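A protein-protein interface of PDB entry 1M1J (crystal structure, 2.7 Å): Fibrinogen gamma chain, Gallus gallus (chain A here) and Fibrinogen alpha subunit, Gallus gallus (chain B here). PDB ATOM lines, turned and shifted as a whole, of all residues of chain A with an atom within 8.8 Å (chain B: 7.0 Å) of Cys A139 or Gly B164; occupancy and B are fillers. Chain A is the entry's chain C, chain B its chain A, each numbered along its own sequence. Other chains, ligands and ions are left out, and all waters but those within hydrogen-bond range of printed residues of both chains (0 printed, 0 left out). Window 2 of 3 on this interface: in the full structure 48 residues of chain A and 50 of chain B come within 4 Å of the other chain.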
ATOM      1  N   HIS A 134      19.307  26.187   6.725  1.00  0.00           N
ATOM      2  CA  HIS A 134      18.743  25.037   6.000  1.00  0.00           C
ATOM      3  C   HIS A 134      19.805  24.100   5.411  1.00  0.00           C
ATOM      4  O   HIS A 134      19.459  23.173   4.700  1.00  0.00           O
ATOM      5  CB  HIS A 134      17.837  25.496   4.846  1.00  0.00           C
ATOM      6  CG  HIS A 134      16.624  26.252   5.286  1.00  0.00           C
ATOM      7  ND1 HIS A 134      15.703  25.731   6.170  1.00  0.00           N
ATOM      8  CD2 HIS A 134      16.193  27.500   4.983  1.00  0.00           C
ATOM      9  CE1 HIS A 134      14.760  26.629   6.398  1.00  0.00           C
ATOM     10  NE2 HIS A 134      15.035  27.710   5.690  1.00  0.00           N
ATOM     11  N   CYS A 135      21.088  24.351   5.690  1.00  0.00           N
ATOM     12  CA  CYS A 135      22.172  23.528   5.160  1.00  0.00           C
ATOM     13  C   CYS A 135      23.095  23.062   6.257  1.00  0.00           C
ATOM     14  O   CYS A 135      24.304  23.308   6.214  1.00  0.00           O
ATOM     15  CB  CYS A 135      22.971  24.310   4.118  1.00  0.00           C
ATOM     16  SG  CYS A 135      21.913  24.856   2.754  1.00  0.00           S
ATOM     17  N   GLN A 136      22.521  22.382   7.237  1.00  0.00           N
ATOM     18  CA  GLN A 136      23.276  21.871   8.367  1.00  0.00           C
ATOM     19  C   GLN A 136      23.009  20.386   8.529  1.00  0.00           C
ATOM     20  O   GLN A 136      23.665  19.706   9.307  1.00  0.00           O
ATOM     21  CB  GLN A 136      22.863  22.605   9.651  1.00  0.00           C
ATOM     22  CG  GLN A 136      23.135  24.088   9.601  1.00  0.00           C
ATOM     23  CD  GLN A 136      24.613  24.392   9.448  1.00  0.00           C
ATOM     24  OE1 GLN A 136      25.009  25.169   8.583  1.00  0.00           O
ATOM     25  NE2 GLN A 136      25.435  23.780  10.293  1.00  0.00           N
ATOM     26  N   GLU A 137      22.024  19.883   7.804  1.00  0.00           N
ATOM     27  CA  GLU A 137      21.690  18.475   7.910  1.00  0.00           C
ATOM     28  C   GLU A 137      22.382  17.692   6.819  1.00  0.00           C
ATOM     29  O   GLU A 137      22.691  18.231   5.754  1.00  0.00           O
ATOM     30  CB  GLU A 137      20.173  18.285   7.820  1.00  0.00           C
ATOM     31  CG  GLU A 137      19.443  18.746   9.063  1.00  0.00           C
ATOM     32  CD  GLU A 137      19.866  17.976  10.298  1.00  0.00           C
ATOM     33  OE1 GLU A 137      19.528  16.774  10.396  1.00  0.00           O
ATOM     34  OE2 GLU A 137      20.543  18.570  11.167  1.00  0.00           O
ATOM     35  N   PRO A 138      22.659  16.411   7.078  1.00  0.00           N
ATOM     36  CA  PRO A 138      23.328  15.557   6.088  1.00  0.00           C
ATOM     37  C   PRO A 138      22.322  15.029   5.094  1.00  0.00           C
ATOM     38  O   PRO A 138      21.115  15.246   5.261  1.00  0.00           O
ATOM     39  CB  PRO A 138      23.929  14.441   6.946  1.00  0.00           C
ATOM     40  CG  PRO A 138      22.925  14.298   8.046  1.00  0.00           C
ATOM     41  CD  PRO A 138      22.602  15.752   8.398  1.00  0.00           C
ATOM     42  N   CYS A 139      22.805  14.357   4.051  1.00  0.00           N
ATOM     43  CA  CYS A 139      21.892  13.773   3.073  1.00  0.00           C
ATOM     44  C   CYS A 139      21.130  12.667   3.793  1.00  0.00           C
ATOM     45  O   CYS A 139      21.655  12.046   4.728  1.00  0.00           O
ATOM     46  CB  CYS A 139      22.647  13.177   1.881  1.00  0.00           C
ATOM     47  SG  CYS A 139      23.732  14.328   0.964  1.00  0.00           S
ATOM     48  N   LYS A 140      19.887  12.435   3.385  1.00  0.00           N
ATOM     49  CA  LYS A 140      19.087  11.396   4.025  1.00  0.00           C
ATOM     50  C   LYS A 140      19.485  10.038   3.433  1.00  0.00           C
ATOM     51  O   LYS A 140      19.390   9.829   2.219  1.00  0.00           O
ATOM     52  CB  LYS A 140      17.586  11.680   3.817  1.00  0.00           C
ATOM     53  CG  LYS A 140      16.653  10.660   4.465  1.00  0.00           C
ATOM     54  CD  LYS A 140      16.803  10.627   5.987  1.00  0.00           C
ATOM     55  CE  LYS A 140      16.089   9.420   6.594  1.00  0.00           C
ATOM     56  NZ  LYS A 140      14.635   9.391   6.260  1.00  0.00           N
ATOM     57  N   ASP A 141      19.941   9.127   4.292  1.00  0.00           N
ATOM     58  CA  ASP A 141      20.368   7.800   3.856  1.00  0.00           C
ATOM     59  C   ASP A 141      19.224   6.791   3.800  1.00  0.00           C
ATOM     60  O   ASP A 141      18.581   6.506   4.808  1.00  0.00           O
ATOM     61  CB  ASP A 141      21.477   7.273   4.776  1.00  0.00           C
ATOM     62  CG  ASP A 141      22.077   5.961   4.280  1.00  0.00           C
ATOM     63  OD1 ASP A 141      21.976   5.659   3.067  1.00  0.00           O
ATOM     64  OD2 ASP A 141      22.666   5.234   5.105  1.00  0.00           O
ATOM     65  N   THR A 142      18.985   6.235   2.615  1.00  0.00           N
ATOM     66  CA  THR A 142      17.912   5.269   2.445  1.00  0.00           C
ATOM     67  C   THR A 142      18.175   3.948   3.143  1.00  0.00           C
ATOM     68  O   THR A 142      17.244   3.264   3.540  1.00  0.00           O
ATOM     69  CB  THR A 142      17.659   4.972   0.965  1.00  0.00           C
ATOM     70  OG1 THR A 142      18.865   4.492   0.353  1.00  0.00           O
ATOM     71  CG2 THR A 142      17.198   6.228   0.255  1.00  0.00           C
ATOM     72  N   ILE B 159      27.122  29.223   0.617  1.00  0.00           N
ATOM     73  CA  ILE B 159      26.279  28.642  -0.424  1.00  0.00           C
ATOM     74  C   ILE B 159      26.785  27.253  -0.800  1.00  0.00           C
ATOM     75  O   ILE B 159      26.000  26.329  -1.039  1.00  0.00           O
ATOM     76  CB  ILE B 159      26.274  29.480  -1.710  1.00  0.00           C
ATOM     77  CG1 ILE B 159      25.338  30.683  -1.558  1.00  0.00           C
ATOM     78  CG2 ILE B 159      25.829  28.608  -2.883  1.00  0.00           C
ATOM     79  CD1 ILE B 159      25.233  31.555  -2.815  1.00  0.00           C
ATOM     80  N   ARG B 160      28.105  27.108  -0.855  1.00  0.00           N
ATOM     81  CA  ARG B 160      28.693  25.837  -1.216  1.00  0.00           C
ATOM     82  C   ARG B 160      28.437  24.779  -0.146  1.00  0.00           C
ATOM     83  O   ARG B 160      28.347  23.598  -0.455  1.00  0.00           O
ATOM     84  CB  ARG B 160      30.200  26.002  -1.469  1.00  0.00           C
ATOM     85  CG  ARG B 160      30.869  24.726  -1.978  1.00  0.00           C
ATOM     86  CD  ARG B 160      32.259  24.977  -2.542  1.00  0.00           C
ATOM     87  NE  ARG B 160      32.276  25.981  -3.607  1.00  0.00           N
ATOM     88  CZ  ARG B 160      32.663  27.249  -3.430  1.00  0.00           C
ATOM     89  NH1 ARG B 160      33.057  27.675  -2.226  1.00  0.00           N
ATOM     90  NH2 ARG B 160      32.693  28.086  -4.462  1.00  0.00           N
ATOM     91  N   ALA B 161      28.310  25.194   1.108  1.00  0.00           N
ATOM     92  CA  ALA B 161      28.063  24.240   2.175  1.00  0.00           C
ATOM     93  C   ALA B 161      26.659  23.647   2.098  1.00  0.00           C
ATOM     94  O   ALA B 161      26.252  22.879   2.969  1.00  0.00           O
ATOM     95  CB  ALA B 161      28.285  24.887   3.528  1.00  0.00           C
ATOM     96  N   CYS B 162      25.909  24.019   1.065  1.00  0.00           N
ATOM     97  CA  CYS B 162      24.578  23.455   0.884  1.00  0.00           C
ATOM     98  C   CYS B 162      24.697  22.217  -0.016  1.00  0.00           C
ATOM     99  O   CYS B 162      23.841  21.330  -0.001  1.00  0.00           O
ATOM    100  CB  CYS B 162      23.625  24.496   0.264  1.00  0.00           C
ATOM    101  SG  CYS B 162      23.105  25.817   1.425  1.00  0.00           S
ATOM    102  N   LYS B 163      25.786  22.149  -0.775  1.00  0.00           N
ATOM    103  CA  LYS B 163      26.037  21.032  -1.679  1.00  0.00           C
ATOM    104  C   LYS B 163      25.889  19.683  -0.988  1.00  0.00           C
ATOM    105  O   LYS B 163      25.539  18.701  -1.617  1.00  0.00           O
ATOM    106  CB  LYS B 163      27.437  21.145  -2.263  1.00  0.00           C
ATOM    107  CG  LYS B 163      27.749  20.205  -3.404  1.00  0.00           C
ATOM    108  CD  LYS B 163      29.263  20.164  -3.642  1.00  0.00           C
ATOM    109  CE  LYS B 163      29.649  19.338  -4.856  1.00  0.00           C
ATOM    110  NZ  LYS B 163      29.224  19.977  -6.131  1.00  0.00           N
ATOM    111  N   GLY B 164      26.146  19.639   0.311  1.00  0.00           N
ATOM    112  CA  GLY B 164      26.027  18.385   1.031  1.00  0.00           C
ATOM    113  C   GLY B 164      24.760  18.278   1.860  1.00  0.00           C
ATOM    114  O   GLY B 164      24.677  17.449   2.763  1.00  0.00           O
ATOM    115  N   SER B 165      23.764  19.104   1.552  1.00  0.00           N
ATOM    116  CA  SER B 165      22.503  19.089   2.290  1.00  0.00           C
ATOM    117  C   SER B 165      21.273  19.091   1.386  1.00  0.00           C
ATOM    118  O   SER B 165      20.264  18.499   1.723  1.00  0.00           O
ATOM    119  CB  SER B 165      22.418  20.302   3.220  1.00  0.00           C
ATOM    120  OG  SER B 165      23.291  20.185   4.325  1.00  0.00           O
ATOM    121  N   CYS B 166      21.390  19.741   0.234  1.00  0.00           N
ATOM    122  CA  CYS B 166      20.302  19.898  -0.718  1.00  0.00           C
ATOM    123  C   CYS B 166      20.445  19.099  -2.024  1.00  0.00           C
ATOM    124  O   CYS B 166      21.541  18.879  -2.528  1.00  0.00           O
ATOM    125  CB  CYS B 166      20.157  21.405  -1.031  1.00  0.00           C
ATOM    126  SG  CYS B 166      20.186  22.462   0.465  1.00  0.00           S
ATOM    127  N   SER B 169      22.938  21.890  -6.291  1.00  0.00           N
ATOM    128  CA  SER B 169      23.872  22.911  -5.859  1.00  0.00           C
ATOM    129  C   SER B 169      24.147  23.973  -6.899  1.00  0.00           C
ATOM    130  O   SER B 169      24.488  23.658  -8.033  1.00  0.00           O
ATOM    131  CB  SER B 169      25.189  22.243  -5.452  1.00  0.00           C
ATOM    132  OG  SER B 169      26.284  23.132  -5.553  1.00  0.00           O
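Among the printed residues, pairs that only touch across the chains: Cys A135 with Ala B161, Cys A135 with Ser B165, Gln A136 with Ser B165 and Glu A137 with Gly B164.
His A134 touches none of the printed residues of chain B. Printed residues of chain B within 4 Å of Gln A136: Ser B165. Of the printed residues of chain B, Glu A137 touches Gly B164 (3.7 Å) and Ser B165 (2.5 Å). Of the printed residues of chain B, Cys A139 touches Gly B164. Printed residues of chain A within 4 Å of Ala B161: Cys A135 (3.8 Å). Of the printed residues of chain A, Cys B162 touches Cys A135. Gly B164 touches just these residues of chain A: Glu A137 (3.7 Å) and Cys A139 (3.7 Å). Of chain A, only Cys A135, Gln A136 and Glu A137 come within 4 Å of Ser B165. The nearest residue of chain A that does not touch Gly B164 is Pro A138 (4.1 Å).
Printed residues of chain A that touch a printed residue of chain B: Cys A135, Gln A136, Glu A137 and Cys A139. Among the printed residues, no Asp or Glu carboxylate lies within 4 Å of a Lys or Arg side-chain nitrogen of the other chain.
O of Gly B164 lies close to SG of Cys A139 (3.7 Å). SG of Cys B166 sits close to SG of Cys A135. SG of Cys A135 is disulfide-bonded to SG of Cys B162 (2.0 Å). The side-chain hydroxyl of Ser B165 sits at hydrogen-bond distance from the backbone carbonyl oxygen of Glu A137 (2.5 Å).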
